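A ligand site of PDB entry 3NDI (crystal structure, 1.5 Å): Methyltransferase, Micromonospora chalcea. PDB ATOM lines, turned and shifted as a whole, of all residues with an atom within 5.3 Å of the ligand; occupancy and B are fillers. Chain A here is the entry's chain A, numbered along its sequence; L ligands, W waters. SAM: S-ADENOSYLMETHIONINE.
The backbone carbonyl oxygen (O) of Ala 178 sits at hydrogen-bond distance from a nitrogen (N) of the ligand (2.9 Å). ND2 of Asn 117 is in hydrogen-bond range of O3' of the ligand (3.2 Å). OG1 of Thr 180 lies within hydrogen-bond range of O4' of the ligand, 3.3 Å away. A nitrogen (N3) of the ligand sits close to the backbone NH of Gly 115 (3.2 Å). A nitrogen (N) of the ligand lies within salt-bridge range of the side-chain carboxylate (OE1) of Glu 113 (3.99 Å). The side-chain carboxylate (OE2) of Glu 136 sits at hydrogen-bond distance from an oxygen (O2') of the ligand (2.6 Å). The side-chain amide nitrogen (ND2) of Asn 179 sits at hydrogen-bond distance from an oxygen (O) of the ligand, 2.8 Å away. The backbone carbonyl oxygen of Phe 157 is in hydrogen-bond range of a nitrogen (N6) of the ligand, 3.2 Å away. The side-chain hydroxyl (OG) of Ser 82 is in hydrogen-bond range of an oxygen (OXT) of the ligand (2.7 Å). N6 of the ligand lies within hydrogen-bond range of OH of Tyr 186 (3.0 Å). The backbone NH of Phe 157 is in hydrogen-bond range of a nitrogen (N1) of the ligand, 3.0 Å away. The backbone carbonyl oxygen (O) of Gly 115 is in hydrogen-bond range of a nitrogen (N) of the ligand (2.9 Å). An oxygen (O2') of the ligand lies within hydrogen-bond range of the side-chain hydroxyl (OG) of Ser 138.
The side-chain carboxylate of Glu 226 lies within hydrogen-bond range of the side-chain hydroxyl of Tyr 78. The side-chain carboxylate of Glu 136 sits at hydrogen-bond distance from the backbone NH of Ser 138, 2.9 Å away. A ring nitrogen (ND1) of His 183 sits close to the backbone carbonyl oxygen (O) of Asn 179. The backbone carbonyl oxygen (O) of Phe 135 is in hydrogen-bond range of the backbone NH (N) of Cys 116 (3.2 Å). The side-chain amide nitrogen (ND2) of Asn 117 sits at hydrogen-bond distance from the backbone carbonyl oxygen (O) of Tyr 80 (2.9 Å). The backbone NH (N) of Ser 82 sits at hydrogen-bond distance from the side-chain amide oxygen (OD1) of Asn 117 (2.9 Å). NH1 of Arg 70 sits at hydrogen-bond distance from OH of Tyr 186, at 3.0 Å. The side-chain carboxylate (OE1) of Glu 136 sits at hydrogen-bond distance from the backbone NH (N) of Asn 117.
Phe 74 touches the ligand (CD1 to C2', 3.6 Å). Tyr 78 touches the ligand. Tyr 80 touches the ligand (CE2 to OXT, 3.8 Å). CZ of Phe 92 touches O of the ligand, 3.3 Å away. Ile 114 touches the ligand. O of Phe 135 touches C2 of the ligand, 3.5 Å away. Pro 137 touches the ligand (CD to N3, 3.2 Å). Phe 156 touches the ligand. His 183 touches the ligand. Ile 184 touches the ligand (CD1 to N6, 3.5 Å). Hydrophobic or aromatic side chains that line the ligand: Phe 74, Tyr 78, Tyr 80, Phe 92, Ile 114, Phe 135, Pro 137, Phe 156, Phe 157, Ala 178, His 183, Ile 184 and Tyr 186.
Water W7 bridges an oxygen (OXT) of the ligand (2.7 Å) and a ring nitrogen (NE2) of His 256 (2.9 Å). Water W2 bridges the side-chain carboxylate of Glu 113 (2.7 Å) and a nitrogen (N) of the ligand (2.8 Å). Water W4 lies within hydrogen-bond range of the side-chain hydroxyl (OH) of Tyr 186 and a nitrogen (N7) of the ligand. Water W1 lies within hydrogen-bond range of an oxygen (OXT) of the ligand and the side-chain hydroxyl of Tyr 80. Water W6 bridges the side-chain carboxylate (OE1) of Glu 226 (2.6 Å) and a ring nitrogen (NE2) of His 183 (2.9 Å).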
ATOM      1  N   ARG A  70      -7.845  24.180 -17.648  1.00  0.00           N
ATOM      2  CA  ARG A  70      -7.311  22.815 -17.756  1.00  0.00           C
ATOM      3  C   ARG A  70      -7.128  22.132 -16.408  1.00  0.00           C
ATOM      4  O   ARG A  70      -7.351  20.935 -16.262  1.00  0.00           O
ATOM      5  CB  ARG A  70      -6.036  22.797 -18.591  1.00  0.00           C
ATOM      6  CG  ARG A  70      -4.845  23.569 -17.959  1.00  0.00           C
ATOM      7  CD  ARG A  70      -3.651  23.537 -18.888  1.00  0.00           C
ATOM      8  NE  ARG A  70      -2.489  24.246 -18.352  1.00  0.00           N
ATOM      9  CZ  ARG A  70      -1.339  24.307 -19.027  1.00  0.00           C
ATOM     10  NH1 ARG A  70      -1.218  23.729 -20.214  1.00  0.00           N
ATOM     11  NH2 ARG A  70      -0.336  24.981 -18.491  1.00  0.00           N
ATOM     12  N   PHE A  74      -8.017  18.247 -15.449  1.00  0.00           N
ATOM     13  CA  PHE A  74      -6.899  17.315 -15.534  1.00  0.00           C
ATOM     14  C   PHE A  74      -6.000  17.612 -14.340  1.00  0.00           C
ATOM     15  O   PHE A  74      -5.455  18.711 -14.194  1.00  0.00           O
ATOM     16  CB  PHE A  74      -6.188  17.424 -16.894  1.00  0.00           C
ATOM     17  CG  PHE A  74      -7.112  17.415 -18.088  1.00  0.00           C
ATOM     18  CD1 PHE A  74      -7.872  16.283 -18.366  1.00  0.00           C
ATOM     19  CD2 PHE A  74      -7.249  18.545 -18.883  1.00  0.00           C
ATOM     20  CE1 PHE A  74      -8.737  16.245 -19.437  1.00  0.00           C
ATOM     21  CE2 PHE A  74      -8.136  18.525 -19.984  1.00  0.00           C
ATOM     22  CZ  PHE A  74      -8.881  17.385 -20.219  1.00  0.00           C
ATOM     23  N   TYR A  78      -8.056  12.818 -11.866  1.00  0.00           N
ATOM     24  CA  TYR A  78      -8.732  12.474 -13.108  1.00  0.00           C
ATOM     25  C   TYR A  78      -9.028  10.982 -13.214  1.00  0.00           C
ATOM     26  O   TYR A  78      -8.115  10.174 -13.056  1.00  0.00           O
ATOM     27  CB  TYR A  78      -7.838  12.861 -14.270  1.00  0.00           C
ATOM     28  CG  TYR A  78      -8.470  12.719 -15.646  1.00  0.00           C
ATOM     29  CD1 TYR A  78      -7.988  11.791 -16.556  1.00  0.00           C
ATOM     30  CD2 TYR A  78      -9.486  13.573 -16.035  1.00  0.00           C
ATOM     31  CE1 TYR A  78      -8.546  11.684 -17.833  1.00  0.00           C
ATOM     32  CE2 TYR A  78     -10.031  13.466 -17.292  1.00  0.00           C
ATOM     33  CZ  TYR A  78      -9.557  12.520 -18.177  1.00  0.00           C
ATOM     34  OH  TYR A  78     -10.128  12.445 -19.423  1.00  0.00           O
ATOM     35  N   TYR A  80     -10.413   8.836 -15.667  1.00  0.00           N
ATOM     36  CA  TYR A  80     -10.596   7.958 -16.834  1.00  0.00           C
ATOM     37  C   TYR A  80      -9.405   7.041 -17.018  1.00  0.00           C
ATOM     38  O   TYR A  80      -8.268   7.518 -17.090  1.00  0.00           O
ATOM     39  CB  TYR A  80     -10.657   8.812 -18.107  1.00  0.00           C
ATOM     40  CG  TYR A  80     -10.913   8.022 -19.355  1.00  0.00           C
ATOM     41  CD1 TYR A  80     -12.073   7.248 -19.480  1.00  0.00           C
ATOM     42  CD2 TYR A  80     -10.005   8.016 -20.408  1.00  0.00           C
ATOM     43  CE1 TYR A  80     -12.368   6.516 -20.612  1.00  0.00           C
ATOM     44  CE2 TYR A  80     -10.271   7.282 -21.549  1.00  0.00           C
ATOM     45  CZ  TYR A  80     -11.436   6.535 -21.627  1.00  0.00           C
ATOM     46  OH  TYR A  80     -11.729   5.831 -22.771  1.00  0.00           O
ATOM     47  N   SER A  82      -7.819   4.544 -19.634  1.00  0.00           N
ATOM     48  CA  SER A  82      -7.909   4.119 -21.018  1.00  0.00           C
ATOM     49  C   SER A  82      -8.015   2.596 -21.123  1.00  0.00           C
ATOM     50  O   SER A  82      -8.717   2.092 -21.988  1.00  0.00           O
ATOM     51  CB  SER A  82      -6.673   4.629 -21.767  1.00  0.00           C
ATOM     52  OG  SER A  82      -6.743   6.040 -21.857  1.00  0.00           O
ATOM     53  N   PHE A  92      -4.755   0.257 -29.653  1.00  0.00           N
ATOM     54  CA  PHE A  92      -3.549   1.061 -29.499  1.00  0.00           C
ATOM     55  C   PHE A  92      -2.289   0.201 -29.603  1.00  0.00           C
ATOM     56  O   PHE A  92      -1.296   0.706 -30.101  1.00  0.00           O
ATOM     57  CB  PHE A  92      -3.531   1.795 -28.158  1.00  0.00           C
ATOM     58  CG  PHE A  92      -4.440   2.964 -28.128  1.00  0.00           C
ATOM     59  CD1 PHE A  92      -4.262   4.033 -28.997  1.00  0.00           C
ATOM     60  CD2 PHE A  92      -5.525   2.981 -27.253  1.00  0.00           C
ATOM     61  CE1 PHE A  92      -5.108   5.109 -28.970  1.00  0.00           C
ATOM     62  CE2 PHE A  92      -6.412   4.047 -27.231  1.00  0.00           C
ATOM     63  CZ  PHE A  92      -6.210   5.126 -28.080  1.00  0.00           C
ATOM     64  N   GLU A 113       4.192  10.727 -26.724  1.00  0.00           N
ATOM     65  CA  GLU A 113       2.741  10.674 -26.743  1.00  0.00           C
ATOM     66  C   GLU A 113       2.162  11.758 -25.823  1.00  0.00           C
ATOM     67  O   GLU A 113       2.500  11.831 -24.657  1.00  0.00           O
ATOM     68  CB  GLU A 113       2.202   9.302 -26.317  1.00  0.00           C
ATOM     69  CG  GLU A 113       0.690   9.344 -26.317  1.00  0.00           C
ATOM     70  CD  GLU A 113       0.059   7.998 -26.012  1.00  0.00           C
ATOM     71  OE1 GLU A 113      -1.147   7.852 -26.323  1.00  0.00           O
ATOM     72  OE2 GLU A 113       0.704   7.100 -25.430  1.00  0.00           O
ATOM     73  N   ILE A 114       1.276  12.577 -26.386  1.00  0.00           N
ATOM     74  CA  ILE A 114       0.493  13.555 -25.625  1.00  0.00           C
ATOM     75  C   ILE A 114      -0.772  12.887 -25.115  1.00  0.00           C
ATOM     76  O   ILE A 114      -1.639  12.459 -25.896  1.00  0.00           O
ATOM     77  CB  ILE A 114       0.134  14.788 -26.509  1.00  0.00           C
ATOM     78  CG1 ILE A 114       1.363  15.318 -27.254  1.00  0.00           C
ATOM     79  CG2 ILE A 114      -0.756  15.754 -25.719  1.00  0.00           C
ATOM     80  CD1 ILE A 114       1.064  16.489 -28.204  1.00  0.00           C
ATOM     81  N   GLY A 115      -0.890  12.809 -23.793  1.00  0.00           N
ATOM     82  CA  GLY A 115      -2.088  12.240 -23.173  1.00  0.00           C
ATOM     83  C   GLY A 115      -1.987  10.740 -23.028  1.00  0.00           C
ATOM     84  O   GLY A 115      -2.988  10.089 -23.352  1.00  0.00           O
ATOM     85  N   CYS A 116      -0.823  10.243 -22.566  1.00  0.00           N
ATOM     86  CA  CYS A 116      -0.613   8.789 -22.534  1.00  0.00           C
ATOM     87  C   CYS A 116      -1.506   8.058 -21.563  1.00  0.00           C
ATOM     88  O   CYS A 116      -1.623   6.833 -21.692  1.00  0.00           O
ATOM     89  CB  CYS A 116       0.875   8.415 -22.396  1.00  0.00           C
ATOM     90  SG  CYS A 116       1.525   8.882 -20.777  1.00  0.00           S
ATOM     91  N   ASN A 117      -2.113   8.769 -20.613  1.00  0.00           N
ATOM     92  CA  ASN A 117      -3.004   8.121 -19.641  1.00  0.00           C
ATOM     93  C   ASN A 117      -2.266   6.982 -18.935  1.00  0.00           C
ATOM     94  O   ASN A 117      -1.091   7.102 -18.603  1.00  0.00           O
ATOM     95  CB  ASN A 117      -4.356   7.701 -20.289  1.00  0.00           C
ATOM     96  CG  ASN A 117      -5.487   7.460 -19.293  1.00  0.00           C
ATOM     97  OD1 ASN A 117      -5.687   6.314 -18.849  1.00  0.00           O
ATOM     98  ND2 ASN A 117      -6.292   8.510 -18.964  1.00  0.00           N
ATOM     99  N   ILE A 120      -1.626   2.857 -22.151  1.00  0.00           N
ATOM    100  CA  ILE A 120      -2.289   1.948 -23.085  1.00  0.00           C
ATOM    101  C   ILE A 120      -1.582   1.771 -24.438  1.00  0.00           C
ATOM    102  O   ILE A 120      -1.541   0.672 -25.003  1.00  0.00           O
ATOM    103  CB  ILE A 120      -3.779   2.356 -23.272  1.00  0.00           C
ATOM    104  CG1 ILE A 120      -4.579   1.337 -24.089  1.00  0.00           C
ATOM    105  CG2 ILE A 120      -3.957   3.669 -24.036  1.00  0.00           C
ATOM    106  CD1 ILE A 120      -6.078   1.565 -23.961  1.00  0.00           C
ATOM    107  N   PHE A 135       3.466  12.423 -22.100  1.00  0.00           N
ATOM    108  CA  PHE A 135       3.013  13.557 -21.281  1.00  0.00           C
ATOM    109  C   PHE A 135       1.613  13.209 -20.799  1.00  0.00           C
ATOM    110  O   PHE A 135       0.686  12.878 -21.549  1.00  0.00           O
ATOM    111  CB  PHE A 135       2.851  14.819 -22.146  1.00  0.00           C
ATOM    112  CG  PHE A 135       4.120  15.525 -22.461  1.00  0.00           C
ATOM    113  CD1 PHE A 135       4.459  16.659 -21.736  1.00  0.00           C
ATOM    114  CD2 PHE A 135       4.987  15.046 -23.424  1.00  0.00           C
ATOM    115  CE1 PHE A 135       5.635  17.353 -22.001  1.00  0.00           C
ATOM    116  CE2 PHE A 135       6.176  15.724 -23.688  1.00  0.00           C
ATOM    117  CZ  PHE A 135       6.501  16.874 -22.965  1.00  0.00           C
ATOM    118  N   GLU A 136       1.474  13.274 -19.475  1.00  0.00           N
ATOM    119  CA  GLU A 136       0.174  12.989 -18.879  1.00  0.00           C
ATOM    120  C   GLU A 136       0.079  13.893 -17.644  1.00  0.00           C
ATOM    121  O   GLU A 136       0.677  13.580 -16.605  1.00  0.00           O
ATOM    122  CB  GLU A 136       0.126  11.521 -18.423  1.00  0.00           C
ATOM    123  CG  GLU A 136      -1.190  11.044 -17.846  1.00  0.00           C
ATOM    124  CD  GLU A 136      -2.346  11.771 -18.502  1.00  0.00           C
ATOM    125  OE1 GLU A 136      -2.679  11.303 -19.615  1.00  0.00           O
ATOM    126  OE2 GLU A 136      -2.872  12.757 -17.957  1.00  0.00           O
ATOM    127  N   PRO A 137      -0.686  14.989 -17.747  1.00  0.00           N
ATOM    128  CA  PRO A 137      -0.768  15.898 -16.577  1.00  0.00           C
ATOM    129  C   PRO A 137      -1.601  15.390 -15.407  1.00  0.00           C
ATOM    130  O   PRO A 137      -1.614  16.053 -14.354  1.00  0.00           O
ATOM    131  CB  PRO A 137      -1.396  17.160 -17.186  1.00  0.00           C
ATOM    132  CG  PRO A 137      -2.286  16.569 -18.293  1.00  0.00           C
ATOM    133  CD  PRO A 137      -1.305  15.619 -18.933  1.00  0.00           C
ATOM    134  N   SER A 138      -2.308  14.264 -15.575  1.00  0.00           N
ATOM    135  CA  SER A 138      -3.164  13.722 -14.534  1.00  0.00           C
ATOM    136  C   SER A 138      -2.352  12.651 -13.814  1.00  0.00           C
ATOM    137  O   SER A 138      -2.158  11.533 -14.320  1.00  0.00           O
ATOM    138  CB  SER A 138      -4.491  13.133 -15.079  1.00  0.00           C
ATOM    139  OG  SER A 138      -5.230  14.202 -15.667  1.00  0.00           O
ATOM    140  N   VAL A 141      -3.288   8.601 -13.121  1.00  0.00           N
ATOM    141  CA  VAL A 141      -3.113   7.711 -14.263  1.00  0.00           C
ATOM    142  C   VAL A 141      -1.667   7.716 -14.796  1.00  0.00           C
ATOM    143  O   VAL A 141      -1.189   6.682 -15.267  1.00  0.00           O
ATOM    144  CB  VAL A 141      -4.122   8.033 -15.424  1.00  0.00           C
ATOM    145  CG1 VAL A 141      -5.547   7.710 -15.008  1.00  0.00           C
ATOM    146  CG2 VAL A 141      -3.923   9.483 -15.922  1.00  0.00           C
ATOM    147  N   ASP A 155       2.942  16.532 -16.903  1.00  0.00           N
ATOM    148  CA  ASP A 155       3.004  17.900 -17.395  1.00  0.00           C
ATOM    149  C   ASP A 155       2.014  17.944 -18.543  1.00  0.00           C
ATOM    150  O   ASP A 155       1.794  16.935 -19.215  1.00  0.00           O
ATOM    151  CB  ASP A 155       4.383  18.185 -18.032  1.00  0.00           C
ATOM    152  CG  ASP A 155       5.365  18.805 -17.057  1.00  0.00           C
ATOM    153  OD1 ASP A 155       6.488  18.257 -16.993  1.00  0.00           O
ATOM    154  OD2 ASP A 155       5.000  19.785 -16.391  1.00  0.00           O
ATOM    155  N   PHE A 156       1.408  19.102 -18.772  1.00  0.00           N
ATOM    156  CA  PHE A 156       0.723  19.366 -20.049  1.00  0.00           C
ATOM    157  C   PHE A 156       1.767  19.534 -21.129  1.00  0.00           C
ATOM    158  O   PHE A 156       2.760  20.247 -20.921  1.00  0.00           O
ATOM    159  CB  PHE A 156      -0.042  20.691 -19.887  1.00  0.00           C
ATOM    160  CG  PHE A 156      -1.145  20.602 -18.844  1.00  0.00           C
ATOM    161  CD1 PHE A 156      -2.319  19.945 -19.151  1.00  0.00           C
ATOM    162  CD2 PHE A 156      -0.992  21.127 -17.565  1.00  0.00           C
ATOM    163  CE1 PHE A 156      -3.352  19.856 -18.191  1.00  0.00           C
ATOM    164  CE2 PHE A 156      -1.986  21.045 -16.615  1.00  0.00           C
ATOM    165  CZ  PHE A 156      -3.183  20.396 -16.908  1.00  0.00           C
ATOM    166  N   PHE A 157       1.532  18.972 -22.313  1.00  0.00           N
ATOM    167  CA  PHE A 157       2.304  19.289 -23.493  1.00  0.00           C
ATOM    168  C   PHE A 157       1.820  20.652 -23.982  1.00  0.00           C
ATOM    169  O   PHE A 157       0.622  20.900 -24.075  1.00  0.00           O
ATOM    170  CB  PHE A 157       1.981  18.253 -24.578  1.00  0.00           C
ATOM    171  CG  PHE A 157       2.866  18.414 -25.784  1.00  0.00           C
ATOM    172  CD1 PHE A 157       2.543  19.389 -26.724  1.00  0.00           C
ATOM    173  CD2 PHE A 157       3.985  17.619 -25.983  1.00  0.00           C
ATOM    174  CE1 PHE A 157       3.336  19.580 -27.872  1.00  0.00           C
ATOM    175  CE2 PHE A 157       4.802  17.805 -27.131  1.00  0.00           C
ATOM    176  CZ  PHE A 157       4.489  18.789 -28.074  1.00  0.00           C
ATOM    177  N   ALA A 178      -4.080  10.654 -28.916  1.00  0.00           N
ATOM    178  CA  ALA A 178      -5.386  10.058 -29.188  1.00  0.00           C
ATOM    179  C   ALA A 178      -6.421  10.605 -28.197  1.00  0.00           C
ATOM    180  O   ALA A 178      -6.124  10.551 -26.987  1.00  0.00           O
ATOM    181  CB  ALA A 178      -5.317   8.536 -29.110  1.00  0.00           C
ATOM    182  N   ASN A 179      -7.578  11.056 -28.638  1.00  0.00           N
ATOM    183  CA  ASN A 179      -8.569  11.596 -27.698  1.00  0.00           C
ATOM    184  C   ASN A 179      -7.979  12.604 -26.739  1.00  0.00           C
ATOM    185  O   ASN A 179      -8.328  12.594 -25.614  1.00  0.00           O
ATOM    186  CB  ASN A 179      -9.319  10.427 -26.997  1.00  0.00           C
ATOM    187  CG  ASN A 179      -9.773   9.415 -28.014  1.00  0.00           C
ATOM    188  OD1 ASN A 179     -10.588   9.709 -28.780  1.00  0.00           O
ATOM    189  ND2 ASN A 179      -9.149   8.210 -28.008  1.00  0.00           N
ATOM    190  N   THR A 180      -7.127  13.439 -27.251  1.00  0.00           N
ATOM    191  CA  THR A 180      -6.386  14.383 -26.391  1.00  0.00           C
ATOM    192  C   THR A 180      -6.278  15.731 -27.090  1.00  0.00           C
ATOM    193  O   THR A 180      -6.547  16.753 -26.472  1.00  0.00           O
ATOM    194  CB  THR A 180      -4.969  13.881 -25.963  1.00  0.00           C
ATOM    195  OG1 THR A 180      -5.117  12.693 -25.193  1.00  0.00           O
ATOM    196  CG2 THR A 180      -4.229  14.965 -25.167  1.00  0.00           C
ATOM    197  N   HIS A 183      -9.117  17.979 -26.702  1.00  0.00           N
ATOM    198  CA  HIS A 183      -9.338  18.382 -25.304  1.00  0.00           C
ATOM    199  C   HIS A 183      -8.618  19.696 -24.993  1.00  0.00           C
ATOM    200  O   HIS A 183      -8.765  20.282 -23.907  1.00  0.00           O
ATOM    201  CB  HIS A 183      -8.755  17.361 -24.313  1.00  0.00           C
ATOM    202  CG  HIS A 183      -9.510  16.068 -24.260  1.00  0.00           C
ATOM    203  ND1 HIS A 183      -9.967  15.445 -25.393  1.00  0.00           N
ATOM    204  CD2 HIS A 183      -9.873  15.267 -23.221  1.00  0.00           C
ATOM    205  CE1 HIS A 183     -10.599  14.329 -25.072  1.00  0.00           C
ATOM    206  NE2 HIS A 183     -10.548  14.199 -23.758  1.00  0.00           N
ATOM    207  N   ILE A 184      -7.810  20.164 -25.934  1.00  0.00           N
ATOM    208  CA  ILE A 184      -6.842  21.220 -25.712  1.00  0.00           C
ATOM    209  C   ILE A 184      -7.140  22.507 -26.473  1.00  0.00           C
ATOM    210  O   ILE A 184      -6.866  22.617 -27.673  1.00  0.00           O
ATOM    211  CB  ILE A 184      -5.420  20.749 -26.071  1.00  0.00           C
ATOM    212  CG1 ILE A 184      -4.999  19.635 -25.108  1.00  0.00           C
ATOM    213  CG2 ILE A 184      -4.439  21.898 -25.850  1.00  0.00           C
ATOM    214  CD1 ILE A 184      -3.714  18.895 -25.582  1.00  0.00           C
ATOM    215  N   TYR A 186      -5.691  25.361 -26.360  1.00  0.00           N
ATOM    216  CA  TYR A 186      -4.452  26.062 -26.708  1.00  0.00           C
ATOM    217  C   TYR A 186      -3.669  25.284 -27.743  1.00  0.00           C
ATOM    218  O   TYR A 186      -2.458  25.038 -27.616  1.00  0.00           O
ATOM    219  CB  TYR A 186      -3.634  26.401 -25.445  1.00  0.00           C
ATOM    220  CG  TYR A 186      -3.474  25.226 -24.493  1.00  0.00           C
ATOM    221  CD1 TYR A 186      -4.470  24.922 -23.581  1.00  0.00           C
ATOM    222  CD2 TYR A 186      -2.316  24.459 -24.505  1.00  0.00           C
ATOM    223  CE1 TYR A 186      -4.338  23.836 -22.706  1.00  0.00           C
ATOM    224  CE2 TYR A 186      -2.154  23.373 -23.624  1.00  0.00           C
ATOM    225  CZ  TYR A 186      -3.183  23.076 -22.755  1.00  0.00           C
ATOM    226  OH  TYR A 186      -3.057  22.013 -21.862  1.00  0.00           O
ATOM    227  N   GLU A 226     -14.439  18.582 -21.732  1.00  0.00           N
ATOM    228  CA  GLU A 226     -13.135  18.089 -22.209  1.00  0.00           C
ATOM    229  C   GLU A 226     -13.035  17.983 -23.725  1.00  0.00           C
ATOM    230  O   GLU A 226     -11.933  17.772 -24.263  1.00  0.00           O
ATOM    231  CB  GLU A 226     -12.867  16.689 -21.631  1.00  0.00           C
ATOM    232  CG  GLU A 226     -12.748  16.763 -20.108  1.00  0.00           C
ATOM    233  CD  GLU A 226     -12.498  15.423 -19.452  1.00  0.00           C
ATOM    234  OE1 GLU A 226     -11.937  14.547 -20.152  1.00  0.00           O
ATOM    235  OE2 GLU A 226     -12.850  15.270 -18.255  1.00  0.00           O
ATOM    236  N   HIS A 256     -14.736   4.936 -30.504  1.00  0.00           N
ATOM    237  CA  HIS A 256     -15.305   6.130 -29.917  1.00  0.00           C
ATOM    238  C   HIS A 256     -16.448   6.793 -30.657  1.00  0.00           C
ATOM    239  O   HIS A 256     -16.526   8.021 -30.632  1.00  0.00           O
ATOM    240  CB  HIS A 256     -14.179   7.098 -29.576  1.00  0.00           C
ATOM    241  CG  HIS A 256     -13.401   6.611 -28.392  1.00  0.00           C
ATOM    242  ND1 HIS A 256     -13.984   6.483 -27.151  1.00  0.00           N
ATOM    243  CD2 HIS A 256     -12.104   6.225 -28.262  1.00  0.00           C
ATOM    244  CE1 HIS A 256     -13.086   6.002 -26.303  1.00  0.00           C
ATOM    245  NE2 HIS A 256     -11.935   5.865 -26.942  1.00  0.00           N
HETATM  246  N   SAM L   1      -4.851   8.692 -25.098  1.00  0.00           N
HETATM  247  CA  SAM L   1      -5.796   8.048 -24.144  1.00  0.00           C
HETATM  248  C   SAM L   1      -6.942   7.410 -24.914  1.00  0.00           C
HETATM  249  O   SAM L   1      -7.086   7.668 -26.127  1.00  0.00           O
HETATM  250  OXT SAM L   1      -7.678   6.680 -24.260  1.00  0.00           O
HETATM  251  CB  SAM L   1      -6.372   8.973 -23.093  1.00  0.00           C
HETATM  252  CG  SAM L   1      -7.397   9.965 -23.638  1.00  0.00           C
HETATM  253  SD  SAM L   1      -8.113  10.929 -22.291  1.00  0.00           S
HETATM  254  CE  SAM L   1      -9.823  11.194 -22.852  1.00  0.00           C
HETATM  255  C5' SAM L   1      -7.345  12.566 -22.534  1.00  0.00           C
HETATM  256  C4' SAM L   1      -6.025  12.565 -21.756  1.00  0.00           C
HETATM  257  O4' SAM L   1      -5.413  13.796 -22.100  1.00  0.00           O
HETATM  258  C3' SAM L   1      -6.194  12.610 -20.234  1.00  0.00           C
HETATM  259  O3' SAM L   1      -5.444  11.566 -19.629  1.00  0.00           O
HETATM  260  C2' SAM L   1      -5.603  13.976 -19.867  1.00  0.00           C
HETATM  261  O2' SAM L   1      -4.987  14.079 -18.606  1.00  0.00           O
HETATM  262  C1' SAM L   1      -4.604  14.219 -20.992  1.00  0.00           C
HETATM  263  N9  SAM L   1      -4.298  15.643 -21.248  1.00  0.00           N
HETATM  264  C8  SAM L   1      -5.077  16.748 -21.130  1.00  0.00           C
HETATM  265  N7  SAM L   1      -4.397  17.861 -21.510  1.00  0.00           N
HETATM  266  C5  SAM L   1      -3.165  17.429 -21.929  1.00  0.00           C
HETATM  267  C6  SAM L   1      -2.022  18.070 -22.413  1.00  0.00           C
HETATM  268  N6  SAM L   1      -1.865  19.390 -22.631  1.00  0.00           N
HETATM  269  N1  SAM L   1      -0.941  17.263 -22.665  1.00  0.00           N
HETATM  270  C2  SAM L   1      -0.938  15.896 -22.471  1.00  0.00           C
HETATM  271  N3  SAM L   1      -2.032  15.231 -21.993  1.00  0.00           N
HETATM  272  C4  SAM L   1      -3.092  16.057 -21.744  1.00  0.00           C
HETATM  273  O   HOH W   1     -10.512   8.250 -24.735  1.00  0.00           O
HETATM  274  O   HOH W   2      -3.528   6.495 -26.161  1.00  0.00           O
HETATM  275  O   HOH W   3     -12.436  11.528 -25.085  1.00  0.00           O
HETATM  276  O   HOH W   4      -5.119  20.661 -21.153  1.00  0.00           O
HETATM  277  O   HOH W   5      -2.794   9.978 -26.541  1.00  0.00           O
HETATM  278  O   HOH W   6     -12.664  13.081 -22.151  1.00  0.00           O
HETATM  279  O   HOH W   7      -9.558   5.183 -25.509  1.00  0.00           O
